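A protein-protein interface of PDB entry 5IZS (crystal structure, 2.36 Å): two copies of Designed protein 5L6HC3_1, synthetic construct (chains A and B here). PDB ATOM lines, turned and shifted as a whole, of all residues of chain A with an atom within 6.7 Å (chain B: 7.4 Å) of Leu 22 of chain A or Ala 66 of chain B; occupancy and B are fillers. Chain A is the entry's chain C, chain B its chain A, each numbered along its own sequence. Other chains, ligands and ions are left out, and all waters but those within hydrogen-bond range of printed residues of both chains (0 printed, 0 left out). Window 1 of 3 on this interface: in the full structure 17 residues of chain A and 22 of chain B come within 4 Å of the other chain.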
ATOM      1  N   LEU A  17      24.599 -21.007  -9.730  1.00  0.00           N
ATOM      2  CA  LEU A  17      24.009 -21.716 -10.860  1.00  0.00           C
ATOM      3  C   LEU A  17      22.507 -21.916 -10.677  1.00  0.00           C
ATOM      4  O   LEU A  17      21.733 -21.736 -11.616  1.00  0.00           O
ATOM      5  CB  LEU A  17      24.704 -23.065 -11.061  1.00  0.00           C
ATOM      6  CG  LEU A  17      24.529 -23.765 -12.409  1.00  0.00           C
ATOM      7  CD1 LEU A  17      24.797 -22.789 -13.534  1.00  0.00           C
ATOM      8  CD2 LEU A  17      25.465 -24.964 -12.509  1.00  0.00           C
ATOM      9  N   ALA A  18      22.098 -22.282  -9.463  1.00  0.00           N
ATOM     10  CA  ALA A  18      20.682 -22.469  -9.154  1.00  0.00           C
ATOM     11  C   ALA A  18      19.917 -21.157  -9.298  1.00  0.00           C
ATOM     12  O   ALA A  18      18.779 -21.138  -9.773  1.00  0.00           O
ATOM     13  CB  ALA A  18      20.511 -23.034  -7.750  1.00  0.00           C
ATOM     14  N   ARG A  19      20.559 -20.062  -8.898  1.00  0.00           N
ATOM     15  CA  ARG A  19      19.965 -18.729  -8.984  1.00  0.00           C
ATOM     16  C   ARG A  19      19.666 -18.325 -10.425  1.00  0.00           C
ATOM     17  O   ARG A  19      18.576 -17.840 -10.728  1.00  0.00           O
ATOM     18  CB  ARG A  19      20.883 -17.683  -8.348  1.00  0.00           C
ATOM     19  CG  ARG A  19      20.952 -17.726  -6.828  1.00  0.00           C
ATOM     20  CD  ARG A  19      21.094 -16.318  -6.257  1.00  0.00           C
ATOM     21  NE  ARG A  19      21.643 -16.316  -4.902  1.00  0.00           N
ATOM     22  CZ  ARG A  19      20.925 -16.498  -3.799  1.00  0.00           C
ATOM     23  NH1 ARG A  19      19.616 -16.703  -3.878  1.00  0.00           N
ATOM     24  NH2 ARG A  19      21.518 -16.480  -2.613  1.00  0.00           N
ATOM     25  N   LYS A  20      20.644 -18.523 -11.306  1.00  0.00           N
ATOM     26  CA  LYS A  20      20.503 -18.146 -12.708  1.00  0.00           C
ATOM     27  C   LYS A  20      19.371 -18.926 -13.367  1.00  0.00           C
ATOM     28  O   LYS A  20      18.598 -18.372 -14.146  1.00  0.00           O
ATOM     29  CB  LYS A  20      21.813 -18.373 -13.466  1.00  0.00           C
ATOM     30  CG  LYS A  20      21.751 -17.991 -14.940  1.00  0.00           C
ATOM     31  CD  LYS A  20      21.211 -16.584 -15.131  1.00  0.00           C
ATOM     32  CE  LYS A  20      21.120 -16.213 -16.602  1.00  0.00           C
ATOM     33  NZ  LYS A  20      20.533 -14.860 -16.802  1.00  0.00           N
ATOM     34  N   LEU A  21      19.273 -20.211 -13.040  1.00  0.00           N
ATOM     35  CA  LEU A  21      18.220 -21.059 -13.584  1.00  0.00           C
ATOM     36  C   LEU A  21      16.850 -20.647 -13.055  1.00  0.00           C
ATOM     37  O   LEU A  21      15.872 -20.637 -13.798  1.00  0.00           O
ATOM     38  CB  LEU A  21      18.499 -22.527 -13.266  1.00  0.00           C
ATOM     39  CG  LEU A  21      19.496 -23.175 -14.227  1.00  0.00           C
ATOM     40  CD1 LEU A  21      19.793 -24.614 -13.827  1.00  0.00           C
ATOM     41  CD2 LEU A  21      18.948 -23.110 -15.642  1.00  0.00           C
ATOM     42  N   LEU A  22      16.785 -20.298 -11.773  1.00  0.00           N
ATOM     43  CA  LEU A  22      15.546 -19.794 -11.195  1.00  0.00           C
ATOM     44  C   LEU A  22      15.176 -18.466 -11.843  1.00  0.00           C
ATOM     45  O   LEU A  22      14.005 -18.203 -12.125  1.00  0.00           O
ATOM     46  CB  LEU A  22      15.675 -19.624  -9.682  1.00  0.00           C
ATOM     47  CG  LEU A  22      14.396 -19.177  -8.971  1.00  0.00           C
ATOM     48  CD1 LEU A  22      13.303 -20.227  -9.122  1.00  0.00           C
ATOM     49  CD2 LEU A  22      14.667 -18.880  -7.501  1.00  0.00           C
ATOM     50  N   GLU A  23      16.189 -17.637 -12.076  1.00  0.00           N
ATOM     51  CA  GLU A  23      16.010 -16.362 -12.754  1.00  0.00           C
ATOM     52  C   GLU A  23      15.470 -16.585 -14.165  1.00  0.00           C
ATOM     53  O   GLU A  23      14.641 -15.816 -14.649  1.00  0.00           O
ATOM     54  CB  GLU A  23      17.328 -15.591 -12.799  1.00  0.00           C
ATOM     55  CG  GLU A  23      17.248 -14.256 -13.511  1.00  0.00           C
ATOM     56  CD  GLU A  23      18.558 -13.500 -13.459  1.00  0.00           C
ATOM     57  OE1 GLU A  23      19.108 -13.344 -12.349  1.00  0.00           O
ATOM     58  OE2 GLU A  23      19.040 -13.068 -14.528  1.00  0.00           O
ATOM     59  N   ALA A  24      15.935 -17.652 -14.809  1.00  0.00           N
ATOM     60  CA  ALA A  24      15.452 -18.026 -16.134  1.00  0.00           C
ATOM     61  C   ALA A  24      13.989 -18.453 -16.075  1.00  0.00           C
ATOM     62  O   ALA A  24      13.174 -18.031 -16.892  1.00  0.00           O
ATOM     63  CB  ALA A  24      16.311 -19.140 -16.718  1.00  0.00           C
ATOM     64  N   VAL A  25      13.666 -19.283 -15.090  1.00  0.00           N
ATOM     65  CA  VAL A  25      12.304 -19.763 -14.891  1.00  0.00           C
ATOM     66  C   VAL A  25      11.348 -18.614 -14.578  1.00  0.00           C
ATOM     67  O   VAL A  25      10.224 -18.575 -15.080  1.00  0.00           O
ATOM     68  CB  VAL A  25      12.252 -20.813 -13.763  1.00  0.00           C
ATOM     69  CG1 VAL A  25      10.867 -20.885 -13.140  1.00  0.00           C
ATOM     70  CG2 VAL A  25      12.689 -22.172 -14.292  1.00  0.00           C
ATOM     71  N   ALA A  26      11.808 -17.674 -13.759  1.00  0.00           N
ATOM     72  CA  ALA A  26      11.014 -16.502 -13.405  1.00  0.00           C
ATOM     73  C   ALA A  26      10.702 -15.640 -14.628  1.00  0.00           C
ATOM     74  O   ALA A  26       9.572 -15.177 -14.797  1.00  0.00           O
ATOM     75  CB  ALA A  26      11.733 -15.679 -12.349  1.00  0.00           C
ATOM     76  N   ARG A  27      11.707 -15.435 -15.476  1.00  0.00           N
ATOM     77  CA  ARG A  27      11.545 -14.632 -16.689  1.00  0.00           C
ATOM     78  C   ARG A  27      10.588 -15.294 -17.673  1.00  0.00           C
ATOM     79  O   ARG A  27       9.746 -14.627 -18.272  1.00  0.00           O
ATOM     80  CB  ARG A  27      12.896 -14.390 -17.369  1.00  0.00           C
ATOM     81  CG  ARG A  27      13.641 -13.157 -16.876  1.00  0.00           C
ATOM     82  CD  ARG A  27      15.048 -13.093 -17.464  1.00  0.00           C
ATOM     83  NE  ARG A  27      15.106 -12.350 -18.720  1.00  0.00           N
ATOM     84  CZ  ARG A  27      16.064 -12.501 -19.630  1.00  0.00           C
ATOM     85  NH1 ARG A  27      17.036 -13.384 -19.430  1.00  0.00           N
ATOM     86  NH2 ARG A  27      16.047 -11.781 -20.744  1.00  0.00           N
ATOM     87  N   LEU B  17      18.446 -28.826  -3.034  1.00  0.00           N
ATOM     88  CA  LEU B  17      18.193 -27.619  -3.811  1.00  0.00           C
ATOM     89  C   LEU B  17      17.493 -27.953  -5.126  1.00  0.00           C
ATOM     90  O   LEU B  17      16.441 -27.395  -5.428  1.00  0.00           O
ATOM     91  CB  LEU B  17      19.505 -26.875  -4.069  1.00  0.00           C
ATOM     92  CG  LEU B  17      19.429 -25.364  -4.283  1.00  0.00           C
ATOM     93  CD1 LEU B  17      18.499 -24.717  -3.269  1.00  0.00           C
ATOM     94  CD2 LEU B  17      20.822 -24.768  -4.178  1.00  0.00           C
ATOM     95  N   LYS B  20      13.882 -28.516  -4.627  1.00  0.00           N
ATOM     96  CA  LYS B  20      13.144 -27.278  -4.389  1.00  0.00           C
ATOM     97  C   LYS B  20      12.804 -26.567  -5.695  1.00  0.00           C
ATOM     98  O   LYS B  20      11.649 -26.222  -5.944  1.00  0.00           O
ATOM     99  CB  LYS B  20      13.952 -26.336  -3.495  1.00  0.00           C
ATOM    100  CG  LYS B  20      14.331 -26.912  -2.146  1.00  0.00           C
ATOM    101  CD  LYS B  20      15.602 -26.261  -1.634  1.00  0.00           C
ATOM    102  CE  LYS B  20      15.880 -26.679  -0.207  1.00  0.00           C
ATOM    103  NZ  LYS B  20      17.174 -27.394  -0.059  1.00  0.00           N
ATOM    104  N   LEU B  21      13.826 -26.346  -6.517  1.00  0.00           N
ATOM    105  CA  LEU B  21      13.672 -25.620  -7.773  1.00  0.00           C
ATOM    106  C   LEU B  21      12.758 -26.372  -8.735  1.00  0.00           C
ATOM    107  O   LEU B  21      11.950 -25.766  -9.436  1.00  0.00           O
ATOM    108  CB  LEU B  21      15.036 -25.368  -8.426  1.00  0.00           C
ATOM    109  CG  LEU B  21      15.868 -24.179  -7.934  1.00  0.00           C
ATOM    110  CD1 LEU B  21      16.358 -24.387  -6.506  1.00  0.00           C
ATOM    111  CD2 LEU B  21      17.042 -23.936  -8.876  1.00  0.00           C
ATOM    112  N   ALA B  24       9.212 -25.997  -7.652  1.00  0.00           N
ATOM    113  CA  ALA B  24       8.785 -24.659  -8.044  1.00  0.00           C
ATOM    114  C   ALA B  24       8.421 -24.637  -9.524  1.00  0.00           C
ATOM    115  O   ALA B  24       7.399 -24.078  -9.913  1.00  0.00           O
ATOM    116  CB  ALA B  24       9.873 -23.637  -7.747  1.00  0.00           C
ATOM    117  N   VAL B  25       9.265 -25.261 -10.340  1.00  0.00           N
ATOM    118  CA  VAL B  25       9.018 -25.379 -11.771  1.00  0.00           C
ATOM    119  C   VAL B  25       7.718 -26.132 -12.045  1.00  0.00           C
ATOM    120  O   VAL B  25       6.946 -25.754 -12.928  1.00  0.00           O
ATOM    121  CB  VAL B  25      10.189 -26.093 -12.483  1.00  0.00           C
ATOM    122  CG1 VAL B  25       9.786 -26.544 -13.880  1.00  0.00           C
ATOM    123  CG2 VAL B  25      11.404 -25.182 -12.539  1.00  0.00           C
ATOM    124  N   ARG B  27       5.123 -26.411  -9.967  1.00  0.00           N
ATOM    125  CA  ARG B  27       3.987 -25.641  -9.467  1.00  0.00           C
ATOM    126  C   ARG B  27       3.663 -24.467 -10.384  1.00  0.00           C
ATOM    127  O   ARG B  27       2.507 -24.075 -10.510  1.00  0.00           O
ATOM    128  CB  ARG B  27       4.244 -25.142  -8.042  1.00  0.00           C
ATOM    129  CG  ARG B  27       3.874 -26.146  -6.957  1.00  0.00           C
ATOM    130  CD  ARG B  27       4.405 -25.730  -5.590  1.00  0.00           C
ATOM    131  NE  ARG B  27       3.549 -24.753  -4.922  1.00  0.00           N
ATOM    132  CZ  ARG B  27       4.003 -23.722  -4.215  1.00  0.00           C
ATOM    133  NH1 ARG B  27       5.310 -23.524  -4.093  1.00  0.00           N
ATOM    134  NH2 ARG B  27       3.154 -22.883  -3.636  1.00  0.00           N
ATOM    135  N   LEU B  28       4.684 -23.908 -11.026  1.00  0.00           N
ATOM    136  CA  LEU B  28       4.461 -22.834 -11.987  1.00  0.00           C
ATOM    137  C   LEU B  28       3.815 -23.377 -13.264  1.00  0.00           C
ATOM    138  O   LEU B  28       3.007 -22.698 -13.898  1.00  0.00           O
ATOM    139  CB  LEU B  28       5.775 -22.119 -12.299  1.00  0.00           C
ATOM    140  CG  LEU B  28       6.338 -21.309 -11.128  1.00  0.00           C
ATOM    141  CD1 LEU B  28       7.758 -20.844 -11.407  1.00  0.00           C
ATOM    142  CD2 LEU B  28       5.432 -20.125 -10.813  1.00  0.00           C
ATOM    143  N   LYS B  60       4.721 -15.149  -8.255  1.00  0.00           N
ATOM    144  CA  LYS B  60       5.679 -14.311  -7.543  1.00  0.00           C
ATOM    145  C   LYS B  60       5.985 -14.863  -6.153  1.00  0.00           C
ATOM    146  O   LYS B  60       7.133 -14.831  -5.704  1.00  0.00           O
ATOM    147  CB  LYS B  60       5.149 -12.884  -7.435  1.00  0.00           C
ATOM    148  CG  LYS B  60       6.037 -11.939  -6.643  1.00  0.00           C
ATOM    149  CD  LYS B  60       5.202 -10.860  -5.979  1.00  0.00           C
ATOM    150  CE  LYS B  60       4.090 -11.489  -5.148  1.00  0.00           C
ATOM    151  NZ  LYS B  60       3.035 -10.515  -4.752  1.00  0.00           N
ATOM    152  N   ARG B  61       4.953 -15.359  -5.473  1.00  0.00           N
ATOM    153  CA  ARG B  61       5.129 -15.982  -4.166  1.00  0.00           C
ATOM    154  C   ARG B  61       6.041 -17.197  -4.285  1.00  0.00           C
ATOM    155  O   ARG B  61       6.993 -17.347  -3.522  1.00  0.00           O
ATOM    156  CB  ARG B  61       3.781 -16.383  -3.562  1.00  0.00           C
ATOM    157  CG  ARG B  61       2.875 -15.203  -3.243  1.00  0.00           C
ATOM    158  CD  ARG B  61       1.917 -15.501  -2.098  1.00  0.00           C
ATOM    159  NE  ARG B  61       0.941 -16.534  -2.432  1.00  0.00           N
ATOM    160  CZ  ARG B  61      -0.227 -16.295  -3.021  1.00  0.00           C
ATOM    161  NH1 ARG B  61      -0.563 -15.054  -3.350  1.00  0.00           N
ATOM    162  NH2 ARG B  61      -1.056 -17.296  -3.284  1.00  0.00           N
ATOM    163  N   ILE B  62       5.752 -18.044  -5.268  1.00  0.00           N
ATOM    164  CA  ILE B  62       6.520 -19.260  -5.513  1.00  0.00           C
ATOM    165  C   ILE B  62       7.993 -18.974  -5.824  1.00  0.00           C
ATOM    166  O   ILE B  62       8.885 -19.627  -5.283  1.00  0.00           O
ATOM    167  CB  ILE B  62       5.901 -20.071  -6.669  1.00  0.00           C
ATOM    168  CG1 ILE B  62       4.499 -20.554  -6.285  1.00  0.00           C
ATOM    169  CG2 ILE B  62       6.781 -21.255  -7.035  1.00  0.00           C
ATOM    170  CD1 ILE B  62       3.843 -21.430  -7.329  1.00  0.00           C
ATOM    171  N   VAL B  63       8.238 -17.998  -6.691  1.00  0.00           N
ATOM    172  CA  VAL B  63       9.599 -17.602  -7.045  1.00  0.00           C
ATOM    173  C   VAL B  63      10.358 -17.093  -5.821  1.00  0.00           C
ATOM    174  O   VAL B  63      11.530 -17.427  -5.624  1.00  0.00           O
ATOM    175  CB  VAL B  63       9.603 -16.518  -8.145  1.00  0.00           C
ATOM    176  CG1 VAL B  63      10.949 -15.803  -8.204  1.00  0.00           C
ATOM    177  CG2 VAL B  63       9.250 -17.133  -9.493  1.00  0.00           C
ATOM    178  N   GLU B  64       9.679 -16.300  -4.997  1.00  0.00           N
ATOM    179  CA  GLU B  64      10.283 -15.745  -3.788  1.00  0.00           C
ATOM    180  C   GLU B  64      10.628 -16.836  -2.776  1.00  0.00           C
ATOM    181  O   GLU B  64      11.712 -16.819  -2.192  1.00  0.00           O
ATOM    182  CB  GLU B  64       9.355 -14.708  -3.153  1.00  0.00           C
ATOM    183  CG  GLU B  64       9.714 -13.274  -3.519  1.00  0.00           C
ATOM    184  CD  GLU B  64       8.506 -12.358  -3.585  1.00  0.00           C
ATOM    185  OE1 GLU B  64       7.393 -12.806  -3.236  1.00  0.00           O
ATOM    186  OE2 GLU B  64       8.669 -11.190  -3.996  1.00  0.00           O
ATOM    187  N   GLU B  65       9.707 -17.777  -2.579  1.00  0.00           N
ATOM    188  CA  GLU B  65       9.943 -18.932  -1.713  1.00  0.00           C
ATOM    189  C   GLU B  65      11.205 -19.673  -2.138  1.00  0.00           C
ATOM    190  O   GLU B  65      12.047 -20.017  -1.310  1.00  0.00           O
ATOM    191  CB  GLU B  65       8.751 -19.891  -1.741  1.00  0.00           C
ATOM    192  CG  GLU B  65       7.474 -19.350  -1.128  1.00  0.00           C
ATOM    193  CD  GLU B  65       6.315 -20.325  -1.249  1.00  0.00           C
ATOM    194  OE1 GLU B  65       6.537 -21.467  -1.707  1.00  0.00           O
ATOM    195  OE2 GLU B  65       5.180 -19.946  -0.891  1.00  0.00           O
ATOM    196  N   ALA B  66      11.332 -19.901  -3.443  1.00  0.00           N
ATOM    197  CA  ALA B  66      12.494 -20.580  -4.005  1.00  0.00           C
ATOM    198  C   ALA B  66      13.765 -19.757  -3.813  1.00  0.00           C
ATOM    199  O   ALA B  66      14.844 -20.308  -3.597  1.00  0.00           O
ATOM    200  CB  ALA B  66      12.270 -20.876  -5.479  1.00  0.00           C
ATOM    201  N   GLU B  67      13.627 -18.437  -3.886  1.00  0.00           N
ATOM    202  CA  GLU B  67      14.764 -17.537  -3.713  1.00  0.00           C
ATOM    203  C   GLU B  67      15.315 -17.609  -2.291  1.00  0.00           C
ATOM    204  O   GLU B  67      16.529 -17.568  -2.086  1.00  0.00           O
ATOM    205  CB  GLU B  67      14.369 -16.099  -4.060  1.00  0.00           C
ATOM    206  CG  GLU B  67      15.035 -15.572  -5.324  1.00  0.00           C
ATOM    207  CD  GLU B  67      14.263 -14.435  -5.966  1.00  0.00           C
ATOM    208  OE1 GLU B  67      13.250 -14.000  -5.382  1.00  0.00           O
ATOM    209  OE2 GLU B  67      14.662 -13.982  -7.062  1.00  0.00           O
ATOM    210  N   GLU B  68      14.420 -17.733  -1.314  1.00  0.00           N
ATOM    211  CA  GLU B  68      14.822 -17.814   0.088  1.00  0.00           C
ATOM    212  C   GLU B  68      15.439 -19.177   0.403  1.00  0.00           C
ATOM    213  O   GLU B  68      16.346 -19.278   1.229  1.00  0.00           O
ATOM    214  CB  GLU B  68      13.630 -17.538   1.009  1.00  0.00           C
ATOM    215  CG  GLU B  68      12.879 -16.261   0.656  1.00  0.00           C
ATOM    216  CD  GLU B  68      12.121 -15.665   1.826  1.00  0.00           C
ATOM    217  OE1 GLU B  68      11.235 -16.347   2.384  1.00  0.00           O
ATOM    218  OE2 GLU B  68      12.417 -14.506   2.186  1.00  0.00           O
ATOM    219  N   GLU B  69      14.945 -20.217  -0.268  1.00  0.00           N
ATOM    220  CA  GLU B  69      15.477 -21.570  -0.111  1.00  0.00           C
ATOM    221  C   GLU B  69      16.924 -21.650  -0.599  1.00  0.00           C
ATOM    222  O   GLU B  69      17.777 -22.249   0.058  1.00  0.00           O
ATOM    223  CB  GLU B  69      14.603 -22.578  -0.864  1.00  0.00           C
ATOM    224  CG  GLU B  69      13.333 -22.980  -0.122  1.00  0.00           C
ATOM    225  CD  GLU B  69      12.234 -23.478  -1.051  1.00  0.00           C
ATOM    226  OE1 GLU B  69      12.353 -23.276  -2.276  1.00  0.00           O
ATOM    227  OE2 GLU B  69      11.250 -24.068  -0.554  1.00  0.00           O
ATOM    228  N   ILE B  70      17.188 -21.036  -1.749  1.00  0.00           N
ATOM    229  CA  ILE B  70      18.538 -20.963  -2.299  1.00  0.00           C
ATOM    230  C   ILE B  70      19.452 -20.193  -1.349  1.00  0.00           C
ATOM    231  O   ILE B  70      20.573 -20.617  -1.065  1.00  0.00           O
ATOM    232  CB  ILE B  70      18.546 -20.291  -3.686  1.00  0.00           C
ATOM    233  CG1 ILE B  70      17.934 -21.224  -4.733  1.00  0.00           C
ATOM    234  CG2 ILE B  70      19.961 -19.915  -4.098  1.00  0.00           C
ATOM    235  CD1 ILE B  70      17.787 -20.592  -6.101  1.00  0.00           C
ATOM    236  N   ARG B  71      18.953 -19.065  -0.853  1.00  0.00           N
ATOM    237  CA  ARG B  71      19.685 -18.241   0.100  1.00  0.00           C
ATOM    238  C   ARG B  71      20.042 -19.031   1.359  1.00  0.00           C
ATOM    239  O   ARG B  71      21.123 -18.858   1.919  1.00  0.00           O
ATOM    240  CB  ARG B  71      18.865 -17.005   0.469  1.00  0.00           C
ATOM    241  CG  ARG B  71      19.653 -15.905   1.159  1.00  0.00           C
ATOM    242  CD  ARG B  71      18.857 -14.607   1.156  1.00  0.00           C
ATOM    243  NE  ARG B  71      18.124 -14.435  -0.096  1.00  0.00           N
ATOM    244  CZ  ARG B  71      16.800 -14.342  -0.180  1.00  0.00           C
ATOM    245  NH1 ARG B  71      16.059 -14.394   0.919  1.00  0.00           N
ATOM    246  NH2 ARG B  71      16.219 -14.193  -1.362  1.00  0.00           N
ATOM    247  N   ARG B  72      19.131 -19.899   1.790  1.00  0.00           N
ATOM    248  CA  ARG B  72      19.349 -20.719   2.981  1.00  0.00           C
ATOM    249  C   ARG B  72      20.331 -21.855   2.715  1.00  0.00           C
ATOM    250  O   ARG B  72      21.148 -22.195   3.573  1.00  0.00           O
ATOM    251  CB  ARG B  72      18.026 -21.289   3.493  1.00  0.00           C
ATOM    252  CG  ARG B  72      17.331 -20.405   4.516  1.00  0.00           C
ATOM    253  CD  ARG B  72      16.302 -21.191   5.313  1.00  0.00           C
ATOM    254  NE  ARG B  72      15.241 -21.737   4.471  1.00  0.00           N
ATOM    255  CZ  ARG B  72      14.062 -21.153   4.284  1.00  0.00           C
ATOM    256  NH1 ARG B  72      13.787 -20.001   4.879  1.00  0.00           N
ATOM    257  NH2 ARG B  72      13.155 -21.724   3.501  1.00  0.00           N
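NH2 of Arg 71 of chain B is in hydrogen-bond range of O of Glu 67 of chain B, at 3.5 Å.
The side-chain carboxylate (OE2) of Glu 68 of chain B lies within salt-bridge range of the guanidinium group (NH1) of Arg 71 of chain B (3.9 Å).
O of Ala 18 of chain A touches CD2 of Leu 21 of chain B (3.4 Å).
Ala 18 of chain A touches Ile 70 of chain B.
Arg 19 of chain A touches Glu 67 of chain B (NH1 to O, 3.7 Å).
NH1 of Arg 19 of chain A touches CG2 of Ile 70 of chain B (3.2 Å).
CA of Arg 71 of chain B touches NH2 of Arg 19 of chain A, 3.7 Å away.
O of Val 63 of chain B touches CD2 of Leu 22 of chain A (3.9 Å).
CD2 of Leu 22 of chain A touches CB of Ala 66 of chain B (3.7 Å).
CD2 of Leu 22 of chain A touches N of Glu 67 of chain B (3.8 Å).
Val 25 of chain A touches Val 25 of chain B.
Leu 28 of chain B touches Val 25 of chain A (CD1 to CG1, 3.6 Å).
Lys 20 of chain A touches none of the printed residues of chain B.
Leu 22 of chain A touches four residues of chain B.
Of the printed residues of chain A, Leu 17 of chain B touches Ala 18.
Of the printed residues of chain A, Val 25 of chain B touches Val 25.
Lys 60 of chain B touches none of the printed residues of chain A.
Printed residues of chain A within 4 Å of Val 63 of chain B: Leu 22 (3.9 Å).
Of the printed residues of chain A, Ala 66 of chain B touches Leu 22.
Of the printed residues of chain A, Arg 71 of chain B touches Arg 19.
The nearest residue of chain B that does not touch Leu 22 of chain A is Leu 21 of chain B (4.6 Å).
Of the 20 printed residues of chain B, 9 touch a printed residue of chain A.
Printed residues of chain B that touch a printed residue of chain A: Leu 17, Leu 21, Val 25, Leu 28, Val 63, Ala 66, Glu 67, Ile 70 and Arg 71.
Among the printed residues, no Asp or Glu carboxylate lies within 4 Å of a Lys or Arg side-chain nitrogen of the other chain.
Val 25 of chain B touches its own counterpart, Val 25 of chain A.
Positions printed for both chains: 17, 20, 21, 24, 25 and 27.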
